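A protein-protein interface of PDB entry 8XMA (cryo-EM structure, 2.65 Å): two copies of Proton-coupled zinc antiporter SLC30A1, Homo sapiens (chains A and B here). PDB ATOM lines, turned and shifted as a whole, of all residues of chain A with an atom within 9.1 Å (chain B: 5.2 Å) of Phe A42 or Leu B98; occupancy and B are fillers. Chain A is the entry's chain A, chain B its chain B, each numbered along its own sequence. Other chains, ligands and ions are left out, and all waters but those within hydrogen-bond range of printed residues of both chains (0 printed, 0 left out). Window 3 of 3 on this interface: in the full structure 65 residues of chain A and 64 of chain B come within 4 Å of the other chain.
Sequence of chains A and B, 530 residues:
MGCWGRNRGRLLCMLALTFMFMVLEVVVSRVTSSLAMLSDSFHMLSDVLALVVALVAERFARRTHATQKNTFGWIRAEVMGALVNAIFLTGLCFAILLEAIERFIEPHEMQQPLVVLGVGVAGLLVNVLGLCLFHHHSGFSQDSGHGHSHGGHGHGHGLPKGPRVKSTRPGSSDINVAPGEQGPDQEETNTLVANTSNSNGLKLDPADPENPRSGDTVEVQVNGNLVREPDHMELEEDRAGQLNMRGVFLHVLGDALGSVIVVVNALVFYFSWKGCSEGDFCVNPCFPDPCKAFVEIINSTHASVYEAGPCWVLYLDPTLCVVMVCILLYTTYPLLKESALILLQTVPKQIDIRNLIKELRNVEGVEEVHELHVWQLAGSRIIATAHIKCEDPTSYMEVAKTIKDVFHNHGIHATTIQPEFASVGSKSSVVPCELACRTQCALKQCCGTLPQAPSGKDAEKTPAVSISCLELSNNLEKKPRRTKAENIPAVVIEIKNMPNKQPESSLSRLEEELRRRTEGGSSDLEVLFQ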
ATOM      1  N   PHE A  21      -9.059 -15.441 -14.635  1.00  0.00           N
ATOM      2  CA  PHE A  21      -8.593 -16.341 -13.585  1.00  0.00           C
ATOM      3  C   PHE A  21      -9.608 -17.443 -13.312  1.00  0.00           C
ATOM      4  O   PHE A  21      -9.228 -18.579 -13.013  1.00  0.00           O
ATOM      5  CB  PHE A  21      -8.286 -15.568 -12.304  1.00  0.00           C
ATOM      6  CG  PHE A  21      -7.694 -16.423 -11.224  1.00  0.00           C
ATOM      7  CD1 PHE A  21      -6.446 -16.995 -11.383  1.00  0.00           C
ATOM      8  CD2 PHE A  21      -8.393 -16.674 -10.058  1.00  0.00           C
ATOM      9  CE1 PHE A  21      -5.902 -17.789 -10.395  1.00  0.00           C
ATOM     10  CE2 PHE A  21      -7.856 -17.467  -9.067  1.00  0.00           C
ATOM     11  CZ  PHE A  21      -6.610 -18.027  -9.237  1.00  0.00           C
ATOM     12  N   MET A  22     -10.902 -17.129 -13.407  1.00  0.00           N
ATOM     13  CA  MET A  22     -11.917 -18.172 -13.291  1.00  0.00           C
ATOM     14  C   MET A  22     -11.783 -19.193 -14.415  1.00  0.00           C
ATOM     15  O   MET A  22     -11.905 -20.403 -14.187  1.00  0.00           O
ATOM     16  CB  MET A  22     -13.313 -17.553 -13.298  1.00  0.00           C
ATOM     17  CG  MET A  22     -14.388 -18.436 -12.689  1.00  0.00           C
ATOM     18  SD  MET A  22     -15.907 -17.537 -12.329  1.00  0.00           S
ATOM     19  CE  MET A  22     -15.262 -16.137 -11.420  1.00  0.00           C
ATOM     20  N   VAL A  23     -11.529 -18.720 -15.637  1.00  0.00           N
ATOM     21  CA  VAL A  23     -11.325 -19.630 -16.761  1.00  0.00           C
ATOM     22  C   VAL A  23     -10.092 -20.497 -16.528  1.00  0.00           C
ATOM     23  O   VAL A  23     -10.105 -21.705 -16.794  1.00  0.00           O
ATOM     24  CB  VAL A  23     -11.223 -18.839 -18.078  1.00  0.00           C
ATOM     25  CG1 VAL A  23     -10.713 -19.729 -19.200  1.00  0.00           C
ATOM     26  CG2 VAL A  23     -12.576 -18.252 -18.441  1.00  0.00           C
ATOM     27  N   GLU A  25      -8.830 -21.358 -13.628  1.00  0.00           N
ATOM     28  CA  GLU A  25      -9.164 -22.324 -12.587  1.00  0.00           C
ATOM     29  C   GLU A  25      -9.996 -23.469 -13.147  1.00  0.00           C
ATOM     30  O   GLU A  25      -9.785 -24.633 -12.788  1.00  0.00           O
ATOM     31  CB  GLU A  25      -9.907 -21.629 -11.448  1.00  0.00           C
ATOM     32  CG  GLU A  25      -9.010 -20.870 -10.491  1.00  0.00           C
ATOM     33  CD  GLU A  25      -9.480 -20.971  -9.055  1.00  0.00           C
ATOM     34  OE1 GLU A  25     -10.547 -21.575  -8.821  1.00  0.00           O
ATOM     35  OE2 GLU A  25      -8.789 -20.439  -8.163  1.00  0.00           O
ATOM     36  N   VAL A  26     -10.949 -23.158 -14.027  1.00  0.00           N
ATOM     37  CA  VAL A  26     -11.767 -24.203 -14.639  1.00  0.00           C
ATOM     38  C   VAL A  26     -10.905 -25.132 -15.486  1.00  0.00           C
ATOM     39  O   VAL A  26     -11.068 -26.358 -15.452  1.00  0.00           O
ATOM     40  CB  VAL A  26     -12.908 -23.576 -15.461  1.00  0.00           C
ATOM     41  CG1 VAL A  26     -13.572 -24.622 -16.341  1.00  0.00           C
ATOM     42  CG2 VAL A  26     -13.926 -22.931 -14.537  1.00  0.00           C
ATOM     43  N   SER A  29      -8.878 -27.342 -13.220  1.00  0.00           N
ATOM     44  CA  SER A  29      -9.738 -28.395 -12.691  1.00  0.00           C
ATOM     45  C   SER A  29      -9.984 -29.483 -13.728  1.00  0.00           C
ATOM     46  O   SER A  29      -9.946 -30.676 -13.408  1.00  0.00           O
ATOM     47  CB  SER A  29     -11.065 -27.801 -12.221  1.00  0.00           C
ATOM     48  OG  SER A  29     -11.930 -28.812 -11.734  1.00  0.00           O
ATOM     49  N   LEU A  35     -12.317 -31.987  -8.216  1.00  0.00           N
ATOM     50  CA  LEU A  35     -13.556 -31.229  -8.079  1.00  0.00           C
ATOM     51  C   LEU A  35     -13.408 -30.026  -7.156  1.00  0.00           C
ATOM     52  O   LEU A  35     -14.234 -29.108  -7.220  1.00  0.00           O
ATOM     53  CB  LEU A  35     -14.676 -32.139  -7.571  1.00  0.00           C
ATOM     54  CG  LEU A  35     -15.492 -32.913  -8.611  1.00  0.00           C
ATOM     55  CD1 LEU A  35     -16.191 -31.958  -9.567  1.00  0.00           C
ATOM     56  CD2 LEU A  35     -14.636 -33.917  -9.375  1.00  0.00           C
ATOM     57  N   ALA A  36     -12.385 -30.012  -6.300  1.00  0.00           N
ATOM     58  CA  ALA A  36     -12.190 -28.879  -5.400  1.00  0.00           C
ATOM     59  C   ALA A  36     -11.903 -27.599  -6.176  1.00  0.00           C
ATOM     60  O   ALA A  36     -12.404 -26.525  -5.823  1.00  0.00           O
ATOM     61  CB  ALA A  36     -11.058 -29.178  -4.417  1.00  0.00           C
ATOM     62  N   MET A  37     -11.093 -27.693  -7.234  1.00  0.00           N
ATOM     63  CA  MET A  37     -10.802 -26.516  -8.047  1.00  0.00           C
ATOM     64  C   MET A  37     -12.051 -26.001  -8.748  1.00  0.00           C
ATOM     65  O   MET A  37     -12.265 -24.787  -8.833  1.00  0.00           O
ATOM     66  CB  MET A  37      -9.706 -26.835  -9.061  1.00  0.00           C
ATOM     67  CG  MET A  37      -8.371 -27.146  -8.425  1.00  0.00           C
ATOM     68  SD  MET A  37      -7.737 -25.713  -7.542  1.00  0.00           S
ATOM     69  CE  MET A  37      -6.324 -26.433  -6.723  1.00  0.00           C
ATOM     70  N   LEU A  38     -12.883 -26.905  -9.268  1.00  0.00           N
ATOM     71  CA  LEU A  38     -14.131 -26.476  -9.892  1.00  0.00           C
ATOM     72  C   LEU A  38     -15.049 -25.805  -8.876  1.00  0.00           C
ATOM     73  O   LEU A  38     -15.682 -24.784  -9.175  1.00  0.00           O
ATOM     74  CB  LEU A  38     -14.823 -27.669 -10.552  1.00  0.00           C
ATOM     75  CG  LEU A  38     -16.120 -27.395 -11.314  1.00  0.00           C
ATOM     76  CD1 LEU A  38     -16.173 -28.221 -12.588  1.00  0.00           C
ATOM     77  CD2 LEU A  38     -17.320 -27.697 -10.436  1.00  0.00           C
ATOM     78  N   SER A  39     -15.133 -26.369  -7.669  1.00  0.00           N
ATOM     79  CA  SER A  39     -15.945 -25.758  -6.623  1.00  0.00           C
ATOM     80  C   SER A  39     -15.434 -24.367  -6.273  1.00  0.00           C
ATOM     81  O   SER A  39     -16.223 -23.436  -6.089  1.00  0.00           O
ATOM     82  CB  SER A  39     -15.963 -26.650  -5.382  1.00  0.00           C
ATOM     83  OG  SER A  39     -14.692 -26.671  -4.756  1.00  0.00           O
ATOM     84  N   ASP A  40     -14.112 -24.207  -6.180  1.00  0.00           N
ATOM     85  CA  ASP A  40     -13.544 -22.894  -5.885  1.00  0.00           C
ATOM     86  C   ASP A  40     -13.819 -21.906  -7.013  1.00  0.00           C
ATOM     87  O   ASP A  40     -14.131 -20.734  -6.764  1.00  0.00           O
ATOM     88  CB  ASP A  40     -12.042 -23.022  -5.634  1.00  0.00           C
ATOM     89  CG  ASP A  40     -11.467 -21.822  -4.911  1.00  0.00           C
ATOM     90  OD1 ASP A  40     -12.236 -20.890  -4.592  1.00  0.00           O
ATOM     91  OD2 ASP A  40     -10.244 -21.811  -4.660  1.00  0.00           O
ATOM     92  N   SER A  41     -13.708 -22.360  -8.264  1.00  0.00           N
ATOM     93  CA  SER A  41     -13.967 -21.480  -9.397  1.00  0.00           C
ATOM     94  C   SER A  41     -15.415 -21.007  -9.397  1.00  0.00           C
ATOM     95  O   SER A  41     -15.696 -19.833  -9.660  1.00  0.00           O
ATOM     96  CB  SER A  41     -13.632 -22.192 -10.707  1.00  0.00           C
ATOM     97  OG  SER A  41     -14.346 -23.409 -10.822  1.00  0.00           O
ATOM     98  N   PHE A  42     -16.350 -21.912  -9.103  1.00  0.00           N
ATOM     99  CA  PHE A  42     -17.747 -21.506  -9.014  1.00  0.00           C
ATOM    100  C   PHE A  42     -18.043 -20.666  -7.778  1.00  0.00           C
ATOM    101  O   PHE A  42     -18.970 -19.851  -7.814  1.00  0.00           O
ATOM    102  CB  PHE A  42     -18.660 -22.733  -9.044  1.00  0.00           C
ATOM    103  CG  PHE A  42     -19.094 -23.128 -10.426  1.00  0.00           C
ATOM    104  CD1 PHE A  42     -19.640 -22.188 -11.284  1.00  0.00           C
ATOM    105  CD2 PHE A  42     -18.960 -24.432 -10.865  1.00  0.00           C
ATOM    106  CE1 PHE A  42     -20.043 -22.542 -12.558  1.00  0.00           C
ATOM    107  CE2 PHE A  42     -19.362 -24.793 -12.138  1.00  0.00           C
ATOM    108  CZ  PHE A  42     -19.904 -23.847 -12.985  1.00  0.00           C
ATOM    109  N   HIS A  43     -17.255 -20.799  -6.717  1.00  0.00           N
ATOM    110  CA  HIS A  43     -17.449 -19.939  -5.548  1.00  0.00           C
ATOM    111  C   HIS A  43     -16.886 -18.549  -5.803  1.00  0.00           C
ATOM    112  O   HIS A  43     -17.298 -17.583  -5.161  1.00  0.00           O
ATOM    113  CB  HIS A  43     -16.792 -20.545  -4.307  1.00  0.00           C
ATOM    114  CG  HIS A  43     -17.283 -21.917  -3.969  1.00  0.00           C
ATOM    115  ND1 HIS A  43     -16.443 -22.927  -3.554  1.00  0.00           N
ATOM    116  CD2 HIS A  43     -18.527 -22.450  -3.996  1.00  0.00           C
ATOM    117  CE1 HIS A  43     -17.150 -24.022  -3.333  1.00  0.00           C
ATOM    118  NE2 HIS A  43     -18.417 -23.759  -3.595  1.00  0.00           N
ATOM    119  N   MET A  44     -15.950 -18.439  -6.739  1.00  0.00           N
ATOM    120  CA  MET A  44     -15.317 -17.164  -7.043  1.00  0.00           C
ATOM    121  C   MET A  44     -16.285 -16.145  -7.640  1.00  0.00           C
ATOM    122  O   MET A  44     -15.944 -14.960  -7.728  1.00  0.00           O
ATOM    123  CB  MET A  44     -14.128 -17.398  -7.987  1.00  0.00           C
ATOM    124  CG  MET A  44     -13.309 -16.164  -8.326  1.00  0.00           C
ATOM    125  SD  MET A  44     -11.879 -16.519  -9.358  1.00  0.00           S
ATOM    126  CE  MET A  44     -11.258 -14.863  -9.618  1.00  0.00           C
ATOM    127  N   LEU A  45     -17.496 -16.562  -8.019  1.00  0.00           N
ATOM    128  CA  LEU A  45     -18.467 -15.632  -8.590  1.00  0.00           C
ATOM    129  C   LEU A  45     -18.882 -14.546  -7.605  1.00  0.00           C
ATOM    130  O   LEU A  45     -19.485 -13.546  -8.016  1.00  0.00           O
ATOM    131  CB  LEU A  45     -19.704 -16.390  -9.073  1.00  0.00           C
ATOM    132  CG  LEU A  45     -19.611 -17.018 -10.464  1.00  0.00           C
ATOM    133  CD1 LEU A  45     -20.453 -18.282 -10.543  1.00  0.00           C
ATOM    134  CD2 LEU A  45     -20.034 -16.022 -11.530  1.00  0.00           C
ATOM    135  N   SER A  46     -18.591 -14.727  -6.317  1.00  0.00           N
ATOM    136  CA  SER A  46     -18.860 -13.673  -5.345  1.00  0.00           C
ATOM    137  C   SER A  46     -18.118 -12.396  -5.713  1.00  0.00           C
ATOM    138  O   SER A  46     -18.674 -11.297  -5.615  1.00  0.00           O
ATOM    139  CB  SER A  46     -18.467 -14.139  -3.946  1.00  0.00           C
ATOM    140  OG  SER A  46     -19.263 -15.236  -3.534  1.00  0.00           O
ATOM    141  N   ASP A  47     -16.864 -12.521  -6.151  1.00  0.00           N
ATOM    142  CA  ASP A  47     -16.116 -11.350  -6.590  1.00  0.00           C
ATOM    143  C   ASP A  47     -16.693 -10.757  -7.869  1.00  0.00           C
ATOM    144  O   ASP A  47     -16.666  -9.533  -8.049  1.00  0.00           O
ATOM    145  CB  ASP A  47     -14.642 -11.705  -6.779  1.00  0.00           C
ATOM    146  CG  ASP A  47     -14.024 -12.309  -5.530  1.00  0.00           C
ATOM    147  OD1 ASP A  47     -14.738 -12.432  -4.512  1.00  0.00           O
ATOM    148  OD2 ASP A  47     -12.823 -12.643  -5.557  1.00  0.00           O
ATOM    149  N   VAL A  48     -17.224 -11.595  -8.763  1.00  0.00           N
ATOM    150  CA  VAL A  48     -17.849 -11.081  -9.980  1.00  0.00           C
ATOM    151  C   VAL A  48     -19.053 -10.215  -9.631  1.00  0.00           C
ATOM    152  O   VAL A  48     -19.212  -9.104 -10.149  1.00  0.00           O
ATOM    153  CB  VAL A  48     -18.239 -12.236 -10.917  1.00  0.00           C
ATOM    154  CG1 VAL A  48     -19.151 -11.735 -12.021  1.00  0.00           C
ATOM    155  CG2 VAL A  48     -17.000 -12.878 -11.506  1.00  0.00           C
ATOM    156  N   LEU A  49     -19.916 -10.707  -8.739  1.00  0.00           N
ATOM    157  CA  LEU A  49     -21.037  -9.885  -8.286  1.00  0.00           C
ATOM    158  C   LEU A  49     -20.591  -8.651  -7.510  1.00  0.00           C
ATOM    159  O   LEU A  49     -21.199  -7.587  -7.671  1.00  0.00           O
ATOM    160  CB  LEU A  49     -22.023 -10.695  -7.439  1.00  0.00           C
ATOM    161  CG  LEU A  49     -23.013 -11.628  -8.146  1.00  0.00           C
ATOM    162  CD1 LEU A  49     -22.372 -12.864  -8.743  1.00  0.00           C
ATOM    163  CD2 LEU A  49     -24.121 -12.018  -7.183  1.00  0.00           C
ATOM    164  N   LEU A  92     -19.789 -12.760   3.773  1.00  0.00           N
ATOM    165  CA  LEU A  92     -18.727 -13.682   3.383  1.00  0.00           C
ATOM    166  C   LEU A  92     -17.799 -13.976   4.555  1.00  0.00           C
ATOM    167  O   LEU A  92     -17.326 -15.106   4.712  1.00  0.00           O
ATOM    168  CB  LEU A  92     -17.945 -13.110   2.203  1.00  0.00           C
ATOM    169  CG  LEU A  92     -18.667 -13.128   0.854  1.00  0.00           C
ATOM    170  CD1 LEU A  92     -17.814 -12.479  -0.223  1.00  0.00           C
ATOM    171  CD2 LEU A  92     -19.041 -14.549   0.466  1.00  0.00           C
ATOM    172  N   CYS B  93     -29.791 -17.048  -1.051  1.00  0.00           N
ATOM    173  CA  CYS B  93     -30.376 -17.687  -2.225  1.00  0.00           C
ATOM    174  C   CYS B  93     -29.315 -17.987  -3.273  1.00  0.00           C
ATOM    175  O   CYS B  93     -29.306 -19.072  -3.863  1.00  0.00           O
ATOM    176  CB  CYS B  93     -31.472 -16.801  -2.815  1.00  0.00           C
ATOM    177  SG  CYS B  93     -32.978 -16.723  -1.830  1.00  0.00           S
ATOM    178  N   PHE B  94     -28.408 -17.039  -3.515  1.00  0.00           N
ATOM    179  CA  PHE B  94     -27.327 -17.286  -4.464  1.00  0.00           C
ATOM    180  C   PHE B  94     -26.423 -18.415  -3.986  1.00  0.00           C
ATOM    181  O   PHE B  94     -26.005 -19.265  -4.781  1.00  0.00           O
ATOM    182  CB  PHE B  94     -26.522 -16.007  -4.690  1.00  0.00           C
ATOM    183  CG  PHE B  94     -27.159 -15.056  -5.658  1.00  0.00           C
ATOM    184  CD1 PHE B  94     -27.968 -15.525  -6.678  1.00  0.00           C
ATOM    185  CD2 PHE B  94     -26.951 -13.692  -5.550  1.00  0.00           C
ATOM    186  CE1 PHE B  94     -28.557 -14.653  -7.572  1.00  0.00           C
ATOM    187  CE2 PHE B  94     -27.538 -12.815  -6.441  1.00  0.00           C
ATOM    188  CZ  PHE B  94     -28.342 -13.297  -7.453  1.00  0.00           C
ATOM    189  N   ALA B  95     -26.117 -18.444  -2.687  1.00  0.00           N
ATOM    190  CA  ALA B  95     -25.261 -19.496  -2.151  1.00  0.00           C
ATOM    191  C   ALA B  95     -25.905 -20.870  -2.298  1.00  0.00           C
ATOM    192  O   ALA B  95     -25.240 -21.837  -2.684  1.00  0.00           O
ATOM    193  CB  ALA B  95     -24.936 -19.211  -0.685  1.00  0.00           C
ATOM    194  N   ILE B  96     -27.202 -20.978  -2.003  1.00  0.00           N
ATOM    195  CA  ILE B  96     -27.842 -22.286  -2.093  1.00  0.00           C
ATOM    196  C   ILE B  96     -28.085 -22.675  -3.546  1.00  0.00           C
ATOM    197  O   ILE B  96     -28.096 -23.863  -3.877  1.00  0.00           O
ATOM    198  CB  ILE B  96     -29.135 -22.328  -1.256  1.00  0.00           C
ATOM    199  CG1 ILE B  96     -30.159 -21.323  -1.766  1.00  0.00           C
ATOM    200  CG2 ILE B  96     -28.829 -22.071   0.210  1.00  0.00           C
ATOM    201  CD1 ILE B  96     -31.517 -21.486  -1.131  1.00  0.00           C
ATOM    202  N   LEU B  97     -28.250 -21.699  -4.444  1.00  0.00           N
ATOM    203  CA  LEU B  97     -28.285 -22.014  -5.870  1.00  0.00           C
ATOM    204  C   LEU B  97     -26.947 -22.565  -6.342  1.00  0.00           C
ATOM    205  O   LEU B  97     -26.896 -23.536  -7.108  1.00  0.00           O
ATOM    206  CB  LEU B  97     -28.662 -20.769  -6.671  1.00  0.00           C
ATOM    207  CG  LEU B  97     -28.797 -20.948  -8.182  1.00  0.00           C
ATOM    208  CD1 LEU B  97     -29.915 -21.918  -8.507  1.00  0.00           C
ATOM    209  CD2 LEU B  97     -29.033 -19.608  -8.854  1.00  0.00           C
ATOM    210  N   LEU B  98     -25.849 -21.955  -5.893  1.00  0.00           N
ATOM    211  CA  LEU B  98     -24.526 -22.462  -6.235  1.00  0.00           C
ATOM    212  C   LEU B  98     -24.319 -23.864  -5.673  1.00  0.00           C
ATOM    213  O   LEU B  98     -23.740 -24.733  -6.336  1.00  0.00           O
ATOM    214  CB  LEU B  98     -23.459 -21.500  -5.718  1.00  0.00           C
ATOM    215  CG  LEU B  98     -22.003 -21.818  -6.033  1.00  0.00           C
ATOM    216  CD1 LEU B  98     -21.791 -21.794  -7.533  1.00  0.00           C
ATOM    217  CD2 LEU B  98     -21.093 -20.818  -5.346  1.00  0.00           C
ATOM    218  N   GLU B  99     -24.797 -24.104  -4.451  1.00  0.00           N
ATOM    219  CA  GLU B  99     -24.703 -25.439  -3.870  1.00  0.00           C
ATOM    220  C   GLU B  99     -25.531 -26.445  -4.665  1.00  0.00           C
ATOM    221  O   GLU B  99     -25.119 -27.595  -4.845  1.00  0.00           O
ATOM    222  CB  GLU B  99     -25.147 -25.407  -2.409  1.00  0.00           C
ATOM    223  CG  GLU B  99     -25.043 -26.744  -1.693  1.00  0.00           C
ATOM    224  CD  GLU B  99     -23.609 -27.223  -1.557  1.00  0.00           C
ATOM    225  OE1 GLU B  99     -22.693 -26.373  -1.551  1.00  0.00           O
ATOM    226  OE2 GLU B  99     -23.395 -28.448  -1.446  1.00  0.00           O
ATOM    227  N   ALA B 100     -26.710 -26.035  -5.135  1.00  0.00           N
ATOM    228  CA  ALA B 100     -27.519 -26.913  -5.974  1.00  0.00           C
ATOM    229  C   ALA B 100     -26.796 -27.244  -7.272  1.00  0.00           C
ATOM    230  O   ALA B 100     -26.857 -28.380  -7.755  1.00  0.00           O
ATOM    231  CB  ALA B 100     -28.873 -26.269  -6.263  1.00  0.00           C
ATOM    232  N   ILE B 101     -26.108 -26.261  -7.852  1.00  0.00           N
ATOM    233  CA  ILE B 101     -25.276 -26.532  -9.023  1.00  0.00           C
ATOM    234  C   ILE B 101     -24.194 -27.548  -8.679  1.00  0.00           C
ATOM    235  O   ILE B 101     -23.894 -28.454  -9.469  1.00  0.00           O
ATOM    236  CB  ILE B 101     -24.673 -25.223  -9.569  1.00  0.00           C
ATOM    237  CG1 ILE B 101     -25.779 -24.291 -10.066  1.00  0.00           C
ATOM    238  CG2 ILE B 101     -23.689 -25.513 -10.687  1.00  0.00           C
ATOM    239  CD1 ILE B 101     -26.604 -24.872 -11.189  1.00  0.00           C
ATOM    240  N   GLU B 102     -23.594 -27.416  -7.493  1.00  0.00           N
ATOM    241  CA  GLU B 102     -22.571 -28.369  -7.069  1.00  0.00           C
ATOM    242  C   GLU B 102     -23.129 -29.785  -6.978  1.00  0.00           C
ATOM    243  O   GLU B 102     -22.503 -30.738  -7.456  1.00  0.00           O
ATOM    244  CB  GLU B 102     -21.978 -27.945  -5.726  1.00  0.00           C
ATOM    245  CG  GLU B 102     -21.040 -26.755  -5.799  1.00  0.00           C
ATOM    246  CD  GLU B 102     -20.448 -26.399  -4.449  1.00  0.00           C
ATOM    247  OE1 GLU B 102     -20.645 -25.253  -3.995  1.00  0.00           O
ATOM    248  OE2 GLU B 102     -19.789 -27.267  -3.840  1.00  0.00           O
ATOM    249  N   ILE B 105     -23.456 -31.203 -10.355  1.00  0.00           N
ATOM    250  CA  ILE B 105     -22.186 -31.652 -10.917  1.00  0.00           C
ATOM    251  C   ILE B 105     -21.759 -32.976 -10.293  1.00  0.00           C
ATOM    252  O   ILE B 105     -21.338 -33.904 -10.996  1.00  0.00           O
ATOM    253  CB  ILE B 105     -21.116 -30.560 -10.743  1.00  0.00           C
ATOM    254  CG1 ILE B 105     -21.395 -29.410 -11.713  1.00  0.00           C
ATOM    255  CG2 ILE B 105     -19.723 -31.126 -10.958  1.00  0.00           C
ATOM    256  CD1 ILE B 105     -20.725 -28.114 -11.342  1.00  0.00           C
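OE1 of Glu B102 is in hydrogen-bond range of NE2 of His A43, at 2.7 Å.
OG of Ser A29 lies within hydrogen-bond range of N of Leu A38 (3.3 Å). OG of Ser A39 lies within hydrogen-bond range of O of Leu A35, at 3.5 Å. The side-chain hydroxyl (OG) of Ser A41 sits at hydrogen-bond distance from the backbone carbonyl oxygen (O) of Leu A38 (2.5 Å). The backbone carbonyl oxygen of Ser A39 lies within hydrogen-bond range of a ring nitrogen (ND1) of His A43, at 2.6 Å. The side-chain hydroxyl of Ser A46 sits at hydrogen-bond distance from the backbone carbonyl oxygen of His A43 (3.5 Å).
Leu A35 touches Ile B105. Leu A38 touches Ile B105 (CD2 to CD1, 3.5 Å). Phe A42 touches Leu B98 (O to CD2, 3.4 Å). Ile B105 touches Phe A42. CD2 of His A43 touches CD2 of Leu B98, at 3.3 Å. Phe B94 touches Leu A49 (CE2 to CD2, 3.6 Å).
Of the printed residues of chain B, Leu A38 touches Ile B105 (3.5 Å). Ser A39 touches none of the printed residues of chain B. Phe A42 touches just these residues of chain B: Leu B98 (3.4 Å) and Ile B105 (3.7 Å). Printed residues of chain B within 4 Å of His A43: Leu B98 and Glu B102. Met A44 touches none of the printed residues of chain B. Of the printed residues of chain B, Leu A49 touches Phe B94. No residue of chain A comes within 4 Å of Leu B97. Of chain A, only Phe A42 and His A43 come within 4 Å of Leu B98. Printed residues of chain A within 4 Å of Glu B102: His A43. Of the printed residues of chain A, Ile B105 touches Leu A35 (3.9 Å), Leu A38 (3.5 Å) and Phe A42 (3.7 Å). The nearest printed residue of chain A that does not touch Ile B105 is Ser A39 (6.9 Å).
Printed residues of chain A that touch a printed residue of chain B: Leu A35, Leu A38, Phe A42, His A43 and Leu A49. Hydrophobic or aromatic side chains of chain A within 4 Å of the printed part of chain B: Leu A35, Leu A38, Phe A42, His A43 and Leu A49. Hydrophobic or aromatic side chains of chain B that line the printed part of chain A: Phe B94, Leu B98 and Ile B105. Along chain B the printed residues that touch a printed residue of chain A span positions 94 to 105. Among the printed residues, 7 pairs touch across the chains. Among the printed residues, no Asp or Glu carboxylate lies within 4 Å of a Lys or Arg side-chain nitrogen of the other chain.
No position is printed for both chains.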
